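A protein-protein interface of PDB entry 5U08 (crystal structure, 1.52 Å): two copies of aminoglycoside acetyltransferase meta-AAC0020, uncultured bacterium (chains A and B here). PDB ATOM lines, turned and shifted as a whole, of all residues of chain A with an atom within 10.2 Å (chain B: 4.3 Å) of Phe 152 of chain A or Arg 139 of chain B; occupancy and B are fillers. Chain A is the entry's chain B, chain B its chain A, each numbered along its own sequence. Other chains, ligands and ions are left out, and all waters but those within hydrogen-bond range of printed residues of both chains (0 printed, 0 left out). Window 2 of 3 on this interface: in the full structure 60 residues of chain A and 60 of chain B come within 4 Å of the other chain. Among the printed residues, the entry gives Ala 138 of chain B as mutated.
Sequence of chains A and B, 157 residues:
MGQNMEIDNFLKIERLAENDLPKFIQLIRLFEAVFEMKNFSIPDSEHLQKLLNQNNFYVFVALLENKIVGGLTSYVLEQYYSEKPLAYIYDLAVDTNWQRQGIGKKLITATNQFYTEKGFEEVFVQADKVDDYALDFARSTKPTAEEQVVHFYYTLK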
ATOM      1  N   TYR A  88     -12.333 -13.165 -35.229  1.00  0.00           N
ATOM      2  CA  TYR A  88     -11.383 -14.267 -35.382  1.00  0.00           C
ATOM      3  C   TYR A  88     -11.062 -14.379 -36.872  1.00  0.00           C
ATOM      4  O   TYR A  88     -11.924 -14.798 -37.656  1.00  0.00           O
ATOM      5  CB  TYR A  88     -12.031 -15.550 -34.854  1.00  0.00           C
ATOM      6  CG  TYR A  88     -11.281 -16.851 -34.955  1.00  0.00           C
ATOM      7  CD1 TYR A  88      -9.934 -16.921 -35.274  1.00  0.00           C
ATOM      8  CD2 TYR A  88     -11.924 -18.037 -34.616  1.00  0.00           C
ATOM      9  CE1 TYR A  88      -9.254 -18.152 -35.331  1.00  0.00           C
ATOM     10  CE2 TYR A  88     -11.251 -19.263 -34.681  1.00  0.00           C
ATOM     11  CZ  TYR A  88      -9.930 -19.296 -35.018  1.00  0.00           C
ATOM     12  OH  TYR A  88      -9.245 -20.487 -35.090  1.00  0.00           O
ATOM     13  N   GLN A 126      -4.188 -16.889 -35.827  1.00  0.00           N
ATOM     14  CA  GLN A 126      -3.266 -17.883 -35.302  1.00  0.00           C
ATOM     15  C   GLN A 126      -2.404 -18.486 -36.400  1.00  0.00           C
ATOM     16  O   GLN A 126      -2.749 -18.466 -37.583  1.00  0.00           O
ATOM     17  CB  GLN A 126      -4.019 -19.000 -34.555  1.00  0.00           C
ATOM     18  CG  GLN A 126      -5.000 -18.445 -33.526  1.00  0.00           C
ATOM     19  CD  GLN A 126      -5.454 -19.448 -32.490  1.00  0.00           C
ATOM     20  OE1 GLN A 126      -5.674 -19.090 -31.319  1.00  0.00           O
ATOM     21  NE2 GLN A 126      -5.613 -20.706 -32.909  1.00  0.00           N
ATOM     22  N   ASP A 128       0.350 -22.068 -36.860  1.00  0.00           N
ATOM     23  CA  ASP A 128       1.000 -23.223 -36.259  1.00  0.00           C
ATOM     24  C   ASP A 128       2.447 -22.900 -35.913  1.00  0.00           C
ATOM     25  O   ASP A 128       3.154 -22.264 -36.693  1.00  0.00           O
ATOM     26  CB  ASP A 128       0.964 -24.408 -37.221  1.00  0.00           C
ATOM     27  CG  ASP A 128      -0.451 -24.796 -37.604  1.00  0.00           C
ATOM     28  OD1 ASP A 128      -1.362 -24.665 -36.758  1.00  0.00           O
ATOM     29  OD2 ASP A 128      -0.652 -25.231 -38.759  1.00  0.00           O
ATOM     30  N   GLN A 148       1.797 -18.184 -26.731  1.00  0.00           N
ATOM     31  CA  GLN A 148       1.988 -19.592 -27.051  1.00  0.00           C
ATOM     32  C   GLN A 148       0.823 -20.371 -26.465  1.00  0.00           C
ATOM     33  O   GLN A 148       0.585 -20.319 -25.250  1.00  0.00           O
ATOM     34  CB  GLN A 148       3.306 -20.102 -26.467  1.00  0.00           C
ATOM     35  CG  GLN A 148       4.458 -19.132 -26.694  1.00  0.00           C
ATOM     36  CD  GLN A 148       4.978 -19.213 -28.097  1.00  0.00           C
ATOM     37  OE1 GLN A 148       5.265 -20.288 -28.634  1.00  0.00           O
ATOM     38  NE2 GLN A 148       5.077 -18.064 -28.721  1.00  0.00           N
ATOM     39  N   VAL A 149       0.107 -21.105 -27.322  1.00  0.00           N
ATOM     40  CA  VAL A 149      -1.056 -21.870 -26.893  1.00  0.00           C
ATOM     41  C   VAL A 149      -0.963 -23.288 -27.466  1.00  0.00           C
ATOM     42  O   VAL A 149      -0.159 -23.573 -28.361  1.00  0.00           O
ATOM     43  CB  VAL A 149      -2.399 -21.186 -27.260  1.00  0.00           C
ATOM     44  CG1 VAL A 149      -2.457 -19.727 -26.759  1.00  0.00           C
ATOM     45  CG2 VAL A 149      -2.624 -21.150 -28.678  1.00  0.00           C
ATOM     46  N   VAL A 150      -1.755 -24.192 -26.889  1.00  0.00           N
ATOM     47  CA  VAL A 150      -1.861 -25.574 -27.368  1.00  0.00           C
ATOM     48  C   VAL A 150      -3.298 -25.797 -27.822  1.00  0.00           C
ATOM     49  O   VAL A 150      -4.250 -25.493 -27.096  1.00  0.00           O
ATOM     50  CB  VAL A 150      -1.433 -26.600 -26.308  1.00  0.00           C
ATOM     51  CG1 VAL A 150      -1.477 -28.022 -26.902  1.00  0.00           C
ATOM     52  CG2 VAL A 150      -0.029 -26.282 -25.822  1.00  0.00           C
ATOM     53  N   HIS A 151      -3.450 -26.289 -29.049  1.00  0.00           N
ATOM     54  CA  HIS A 151      -4.746 -26.493 -29.689  1.00  0.00           C
ATOM     55  C   HIS A 151      -5.099 -27.980 -29.635  1.00  0.00           C
ATOM     56  O   HIS A 151      -4.285 -28.819 -30.018  1.00  0.00           O
ATOM     57  CB  HIS A 151      -4.625 -25.994 -31.127  1.00  0.00           C
ATOM     58  CG  HIS A 151      -5.799 -26.288 -31.998  1.00  0.00           C
ATOM     59  ND1 HIS A 151      -6.885 -25.442 -32.078  1.00  0.00           N
ATOM     60  CD2 HIS A 151      -6.036 -27.294 -32.872  1.00  0.00           C
ATOM     61  CE1 HIS A 151      -7.746 -25.916 -32.961  1.00  0.00           C
ATOM     62  NE2 HIS A 151      -7.269 -27.053 -33.440  1.00  0.00           N
ATOM     63  N   PHE A 152      -6.299 -28.303 -29.145  1.00  0.00           N
ATOM     64  CA  PHE A 152      -6.741 -29.692 -29.064  1.00  0.00           C
ATOM     65  C   PHE A 152      -7.978 -29.846 -29.920  1.00  0.00           C
ATOM     66  O   PHE A 152      -8.844 -28.966 -29.915  1.00  0.00           O
ATOM     67  CB  PHE A 152      -7.087 -30.071 -27.630  1.00  0.00           C
ATOM     68  CG  PHE A 152      -5.942 -29.979 -26.695  1.00  0.00           C
ATOM     69  CD1 PHE A 152      -5.633 -28.785 -26.029  1.00  0.00           C
ATOM     70  CD2 PHE A 152      -5.170 -31.095 -26.435  1.00  0.00           C
ATOM     71  CE1 PHE A 152      -4.551 -28.730 -25.146  1.00  0.00           C
ATOM     72  CE2 PHE A 152      -4.106 -31.044 -25.578  1.00  0.00           C
ATOM     73  CZ  PHE A 152      -3.792 -29.906 -24.907  1.00  0.00           C
ATOM     74  N   TYR A 153      -8.072 -30.927 -30.704  1.00  0.00           N
ATOM     75  CA  TYR A 153      -9.327 -31.112 -31.412  1.00  0.00           C
ATOM     76  C   TYR A 153      -9.839 -32.523 -31.208  1.00  0.00           C
ATOM     77  O   TYR A 153      -9.085 -33.444 -30.882  1.00  0.00           O
ATOM     78  CB  TYR A 153      -9.246 -30.747 -32.936  1.00  0.00           C
ATOM     79  CG  TYR A 153      -8.338 -31.572 -33.801  1.00  0.00           C
ATOM     80  CD1 TYR A 153      -8.760 -32.799 -34.333  1.00  0.00           C
ATOM     81  CD2 TYR A 153      -7.058 -31.144 -34.101  1.00  0.00           C
ATOM     82  CE1 TYR A 153      -7.934 -33.547 -35.135  1.00  0.00           C
ATOM     83  CE2 TYR A 153      -6.225 -31.888 -34.913  1.00  0.00           C
ATOM     84  CZ  TYR A 153      -6.665 -33.092 -35.425  1.00  0.00           C
ATOM     85  OH  TYR A 153      -5.821 -33.848 -36.219  1.00  0.00           O
ATOM     86  N   TYR A 154     -11.151 -32.653 -31.423  1.00  0.00           N
ATOM     87  CA  TYR A 154     -11.893 -33.903 -31.321  1.00  0.00           C
ATOM     88  C   TYR A 154     -12.569 -34.167 -32.659  1.00  0.00           C
ATOM     89  O   TYR A 154     -13.513 -33.458 -33.018  1.00  0.00           O
ATOM     90  CB  TYR A 154     -12.933 -33.798 -30.201  1.00  0.00           C
ATOM     91  CG  TYR A 154     -12.379 -33.369 -28.855  1.00  0.00           C
ATOM     92  CD1 TYR A 154     -12.392 -32.042 -28.498  1.00  0.00           C
ATOM     93  CD2 TYR A 154     -11.926 -34.304 -27.910  1.00  0.00           C
ATOM     94  CE1 TYR A 154     -11.898 -31.607 -27.279  1.00  0.00           C
ATOM     95  CE2 TYR A 154     -11.446 -33.889 -26.675  1.00  0.00           C
ATOM     96  CZ  TYR A 154     -11.439 -32.530 -26.371  1.00  0.00           C
ATOM     97  OH  TYR A 154     -10.982 -32.031 -25.181  1.00  0.00           O
ATOM     98  N   THR A 155     -12.139 -35.208 -33.369  1.00  0.00           N
ATOM     99  CA  THR A 155     -12.789 -35.555 -34.636  1.00  0.00           C
ATOM    100  C   THR A 155     -14.049 -36.351 -34.319  1.00  0.00           C
ATOM    101  O   THR A 155     -13.960 -37.418 -33.694  1.00  0.00           O
ATOM    102  CB  THR A 155     -11.863 -36.382 -35.518  1.00  0.00           C
ATOM    103  OG1 THR A 155     -10.701 -35.619 -35.890  1.00  0.00           O
ATOM    104  CG2 THR A 155     -12.624 -36.815 -36.770  1.00  0.00           C
ATOM    105  N   LEU A 156     -15.205 -35.858 -34.760  1.00  0.00           N
ATOM    106  CA  LEU A 156     -16.474 -36.456 -34.372  1.00  0.00           C
ATOM    107  C   LEU A 156     -16.855 -37.581 -35.323  1.00  0.00           C
ATOM    108  O   LEU A 156     -16.439 -37.613 -36.479  1.00  0.00           O
ATOM    109  CB  LEU A 156     -17.586 -35.406 -34.326  1.00  0.00           C
ATOM    110  CG  LEU A 156     -17.276 -34.214 -33.422  1.00  0.00           C
ATOM    111  CD1 LEU A 156     -18.502 -33.278 -33.346  1.00  0.00           C
ATOM    112  CD2 LEU A 156     -16.852 -34.619 -32.025  1.00  0.00           C
ATOM    113  N   VAL B 123     -14.736 -30.589 -32.925  1.00  0.00           N
ATOM    114  CA  VAL B 123     -14.783 -29.621 -31.827  1.00  0.00           C
ATOM    115  C   VAL B 123     -13.341 -29.313 -31.454  1.00  0.00           C
ATOM    116  O   VAL B 123     -12.506 -30.220 -31.449  1.00  0.00           O
ATOM    117  CB  VAL B 123     -15.549 -30.193 -30.619  1.00  0.00           C
ATOM    118  CG1 VAL B 123     -15.530 -29.202 -29.458  1.00  0.00           C
ATOM    119  CG2 VAL B 123     -16.988 -30.518 -31.011  1.00  0.00           C
ATOM    120  N   PHE B 124     -13.032 -28.059 -31.126  1.00  0.00           N
ATOM    121  CA  PHE B 124     -11.680 -27.793 -30.663  1.00  0.00           C
ATOM    122  C   PHE B 124     -11.692 -26.879 -29.455  1.00  0.00           C
ATOM    123  O   PHE B 124     -12.668 -26.194 -29.183  1.00  0.00           O
ATOM    124  CB  PHE B 124     -10.772 -27.224 -31.782  1.00  0.00           C
ATOM    125  CG  PHE B 124     -11.191 -25.857 -32.340  1.00  0.00           C
ATOM    126  CD1 PHE B 124     -10.625 -24.701 -31.865  1.00  0.00           C
ATOM    127  CD2 PHE B 124     -12.086 -25.780 -33.386  1.00  0.00           C
ATOM    128  CE1 PHE B 124     -10.977 -23.443 -32.421  1.00  0.00           C
ATOM    129  CE2 PHE B 124     -12.445 -24.538 -33.931  1.00  0.00           C
ATOM    130  CZ  PHE B 124     -11.878 -23.385 -33.440  1.00  0.00           C
ATOM    131  N   VAL B 125     -10.579 -26.911 -28.730  1.00  0.00           N
ATOM    132  CA  VAL B 125     -10.403 -26.139 -27.495  1.00  0.00           C
ATOM    133  C   VAL B 125      -8.914 -25.844 -27.353  1.00  0.00           C
ATOM    134  O   VAL B 125      -8.070 -26.597 -27.847  1.00  0.00           O
ATOM    135  CB  VAL B 125     -10.947 -26.939 -26.277  1.00  0.00           C
ATOM    136  CG1 VAL B 125     -10.110 -28.210 -26.017  1.00  0.00           C
ATOM    137  CG2 VAL B 125     -10.944 -26.081 -24.976  1.00  0.00           C
ATOM    138  N   LEU B 135      -3.669 -27.808 -19.340  1.00  0.00           N
ATOM    139  CA  LEU B 135      -3.122 -28.755 -20.307  1.00  0.00           C
ATOM    140  C   LEU B 135      -3.298 -30.189 -19.849  1.00  0.00           C
ATOM    141  O   LEU B 135      -3.638 -31.065 -20.660  1.00  0.00           O
ATOM    142  CB  LEU B 135      -1.644 -28.482 -20.540  1.00  0.00           C
ATOM    143  CG  LEU B 135      -1.388 -27.189 -21.274  1.00  0.00           C
ATOM    144  CD1 LEU B 135       0.059 -26.944 -21.139  1.00  0.00           C
ATOM    145  CD2 LEU B 135      -1.821 -27.281 -22.752  1.00  0.00           C
ATOM    146  N   ASP B 136      -2.991 -30.458 -18.573  1.00  0.00           N
ATOM    147  CA  ASP B 136      -3.177 -31.805 -18.052  1.00  0.00           C
ATOM    148  C   ASP B 136      -4.628 -32.225 -18.181  1.00  0.00           C
ATOM    149  O   ASP B 136      -4.925 -33.367 -18.556  1.00  0.00           O
ATOM    150  CB  ASP B 136      -2.713 -31.874 -16.595  1.00  0.00           C
ATOM    151  CG  ASP B 136      -1.810 -33.079 -16.329  1.00  0.00           C
ATOM    152  OD1 ASP B 136      -1.040 -33.044 -15.346  1.00  0.00           O
ATOM    153  OD2 ASP B 136      -1.849 -34.053 -17.113  1.00  0.00           O
ATOM    154  N   PHE B 137      -5.547 -31.300 -17.916  1.00  0.00           N
ATOM    155  CA  PHE B 137      -6.956 -31.617 -18.086  1.00  0.00           C
ATOM    156  C   PHE B 137      -7.283 -31.970 -19.536  1.00  0.00           C
ATOM    157  O   PHE B 137      -7.918 -32.997 -19.811  1.00  0.00           O
ATOM    158  CB  PHE B 137      -7.848 -30.455 -17.663  1.00  0.00           C
ATOM    159  CG  PHE B 137      -9.251 -30.680 -18.077  1.00  0.00           C
ATOM    160  CD1 PHE B 137      -9.998 -31.685 -17.486  1.00  0.00           C
ATOM    161  CD2 PHE B 137      -9.781 -30.002 -19.144  1.00  0.00           C
ATOM    162  CE1 PHE B 137     -11.288 -31.945 -17.914  1.00  0.00           C
ATOM    163  CE2 PHE B 137     -11.052 -30.270 -19.585  1.00  0.00           C
ATOM    164  CZ  PHE B 137     -11.806 -31.230 -18.980  1.00  0.00           C
ATOM    165  N   ALA B 138      -6.933 -31.084 -20.478  1.00  0.00           N
ATOM    166  CA  ALA B 138      -7.282 -31.363 -21.865  1.00  0.00           C
ATOM    167  C   ALA B 138      -6.678 -32.675 -22.340  1.00  0.00           C
ATOM    168  O   ALA B 138      -7.310 -33.427 -23.101  1.00  0.00           O
ATOM    169  CB  ALA B 138      -6.805 -30.211 -22.756  1.00  0.00           C
ATOM    170  N   ARG B 139      -5.476 -32.986 -21.875  1.00  0.00           N
ATOM    171  CA  ARG B 139      -4.836 -34.210 -22.338  1.00  0.00           C
ATOM    172  C   ARG B 139      -5.489 -35.446 -21.759  1.00  0.00           C
ATOM    173  O   ARG B 139      -5.143 -36.564 -22.180  1.00  0.00           O
ATOM    174  CB  ARG B 139      -3.346 -34.160 -22.006  1.00  0.00           C
ATOM    175  CG  ARG B 139      -2.588 -33.243 -22.993  1.00  0.00           C
ATOM    176  CD  ARG B 139      -1.290 -32.730 -22.391  1.00  0.00           C
ATOM    177  NE  ARG B 139      -0.627 -31.849 -23.359  1.00  0.00           N
ATOM    178  CZ  ARG B 139       0.392 -31.041 -23.082  1.00  0.00           C
ATOM    179  NH1 ARG B 139       0.809 -30.899 -21.833  1.00  0.00           N
ATOM    180  NH2 ARG B 139       0.918 -30.291 -24.074  1.00  0.00           N
ATOM    181  N   SER B 140      -6.405 -35.283 -20.799  1.00  0.00           N
ATOM    182  CA  SER B 140      -7.105 -36.403 -20.185  1.00  0.00           C
ATOM    183  C   SER B 140      -8.475 -36.669 -20.809  1.00  0.00           C
ATOM    184  O   SER B 140      -9.186 -37.570 -20.348  1.00  0.00           O
ATOM    185  CB  SER B 140      -7.261 -36.153 -18.675  1.00  0.00           C
ATOM    186  OG  SER B 140      -8.338 -35.261 -18.397  1.00  0.00           O
ATOM    187  N   THR B 141      -8.873 -35.907 -21.840  1.00  0.00           N
ATOM    188  CA  THR B 141     -10.189 -36.039 -22.465  1.00  0.00           C
ATOM    189  C   THR B 141     -10.169 -36.811 -23.775  1.00  0.00           C
ATOM    190  O   THR B 141     -11.120 -36.696 -24.563  1.00  0.00           O
ATOM    191  CB  THR B 141     -10.792 -34.659 -22.727  1.00  0.00           C
ATOM    192  OG1 THR B 141      -9.959 -33.919 -23.628  1.00  0.00           O
ATOM    193  CG2 THR B 141     -10.907 -33.906 -21.388  1.00  0.00           C
ATOM    194  N   PRO B 143      -8.394 -36.291 -26.582  1.00  0.00           N
ATOM    195  CA  PRO B 143      -8.410 -35.493 -27.814  1.00  0.00           C
ATOM    196  C   PRO B 143      -7.818 -36.290 -28.968  1.00  0.00           C
ATOM    197  O   PRO B 143      -6.925 -37.137 -28.796  1.00  0.00           O
ATOM    198  CB  PRO B 143      -7.546 -34.276 -27.465  1.00  0.00           C
ATOM    199  CG  PRO B 143      -6.574 -34.816 -26.446  1.00  0.00           C
ATOM    200  CD  PRO B 143      -7.365 -35.815 -25.624  1.00  0.00           C
ATOM    201  N   ALA B 145      -5.996 -35.058 -31.381  1.00  0.00           N
ATOM    202  CA  ALA B 145      -4.641 -34.583 -31.584  1.00  0.00           C
ATOM    203  C   ALA B 145      -4.464 -33.286 -30.820  1.00  0.00           C
ATOM    204  O   ALA B 145      -5.438 -32.650 -30.401  1.00  0.00           O
ATOM    205  CB  ALA B 145      -4.342 -34.341 -33.063  1.00  0.00           C
ATOM    206  N   GLU B 146      -3.195 -32.893 -30.674  1.00  0.00           N
ATOM    207  CA  GLU B 146      -2.852 -31.602 -30.095  1.00  0.00           C
ATOM    208  C   GLU B 146      -1.745 -30.986 -30.931  1.00  0.00           C
ATOM    209  O   GLU B 146      -0.901 -31.695 -31.488  1.00  0.00           O
ATOM    210  CB  GLU B 146      -2.403 -31.716 -28.622  1.00  0.00           C
ATOM    211  CG  GLU B 146      -1.069 -32.382 -28.401  1.00  0.00           C
ATOM    212  CD  GLU B 146      -0.615 -32.334 -26.936  1.00  0.00           C
ATOM    213  OE1 GLU B 146       0.318 -31.564 -26.602  1.00  0.00           O
ATOM    214  OE2 GLU B 146      -1.195 -33.064 -26.108  1.00  0.00           O
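Among the printed residues, pairs that only touch across the chains: Val 150 of chain A with Leu 135 of chain B, Val 150 of chain A with Glu 146 of chain B, His 151 of chain A with Phe 124 of chain B, His 151 of chain A with Val 125 of chain B, His 151 of chain A with Glu 146 of chain B, Phe 152 of chain A with Phe 124 of chain B, Phe 152 of chain A with Leu 135 of chain B, Phe 152 of chain A with Ala 138 of chain B, Phe 152 of chain A with Arg 139 of chain B, Phe 152 of chain A with Pro 143 of chain B, Phe 152 of chain A with Ala 145 of chain B, Phe 152 of chain A with Glu 146 of chain B, Tyr 153 of chain A with Val 123 of chain B, Tyr 153 of chain A with Pro 143 of chain B, Tyr 154 of chain A with Pro 143 of chain B and Leu 156 of chain A with Val 123 of chain B.
No position is printed for both chains.
Of the 20 pairs that touch across the chains among the printed residues, none has its exchanged pair printed and touching as well.
Val 149 of chain A touches none of the printed residues of chain B.
Of chain B, only Phe 124, Val 125, Leu 135, Ala 138, Arg 139, Pro 143, Ala 145 and Glu 146 come within 4 Å of Phe 152 of chain A.
Printed residues of chain B within 4 Å of Tyr 154 of chain A: Val 123 (2.8 Å), Thr 141 (2.7 Å) and Pro 143 (3.6 Å).
Of the printed residues of chain B, Leu 156 of chain A touches Val 123 (3.9 Å).
Printed residues of chain A within 4 Å of Val 125 of chain B: His 151 (3.7 Å) and Phe 152 (2.8 Å).
Leu 135 of chain B touches just these residues of chain A: Val 150 and Phe 152.
Phe 137 of chain B touches none of the printed residues of chain A.
Ala 138 of chain B touches one residue of chain A.
Of chain A, only Phe 152 (3.7 Å) comes within 4 Å of Arg 139 of chain B.
Printed residues of chain A within 4 Å of Thr 141 of chain B: Tyr 154.
Printed residues of chain A within 4 Å of Glu 146 of chain B: Val 150 (3.98 Å), His 151 (3.1 Å) and Phe 152 (3.6 Å).
The backbone carbonyl oxygen of Ala 138 of chain B lies within hydrogen-bond range of the side-chain hydroxyl of Thr 141 of chain B, 2.7 Å away.
OE1 of Glu 146 of chain B lies within salt-bridge range of NH2 of Arg 139 of chain B (2.9 Å).
O of Val 123 of chain B lies within hydrogen-bond range of N of Tyr 154 of chain A (2.8 Å).
The backbone NH (N) of Phe 152 of chain A is in hydrogen-bond range of the backbone carbonyl oxygen (O) of Val 125 of chain B (2.8 Å).
The side-chain hydroxyl (OG1) of Thr 141 of chain B lies within hydrogen-bond range of the side-chain hydroxyl (OH) of Tyr 154 of chain A, 2.7 Å away.
O of Ala 145 of chain B lies within hydrogen-bond range of N of Tyr 153 of chain A, 3.2 Å away.
Of the 12 printed residues of chain A, 6 touch a printed residue of chain B.
Printed residues of chain B that touch a printed residue of chain A: Val 123, Phe 124, Val 125, Leu 135, Ala 138, Arg 139, Thr 141, Pro 143, Ala 145 and Glu 146.
Hydrophobic or aromatic side chains of chain B within 4 Å of the printed part of chain A: Val 123, Phe 124, Val 125, Leu 135, Ala 138, Pro 143 and Ala 145.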
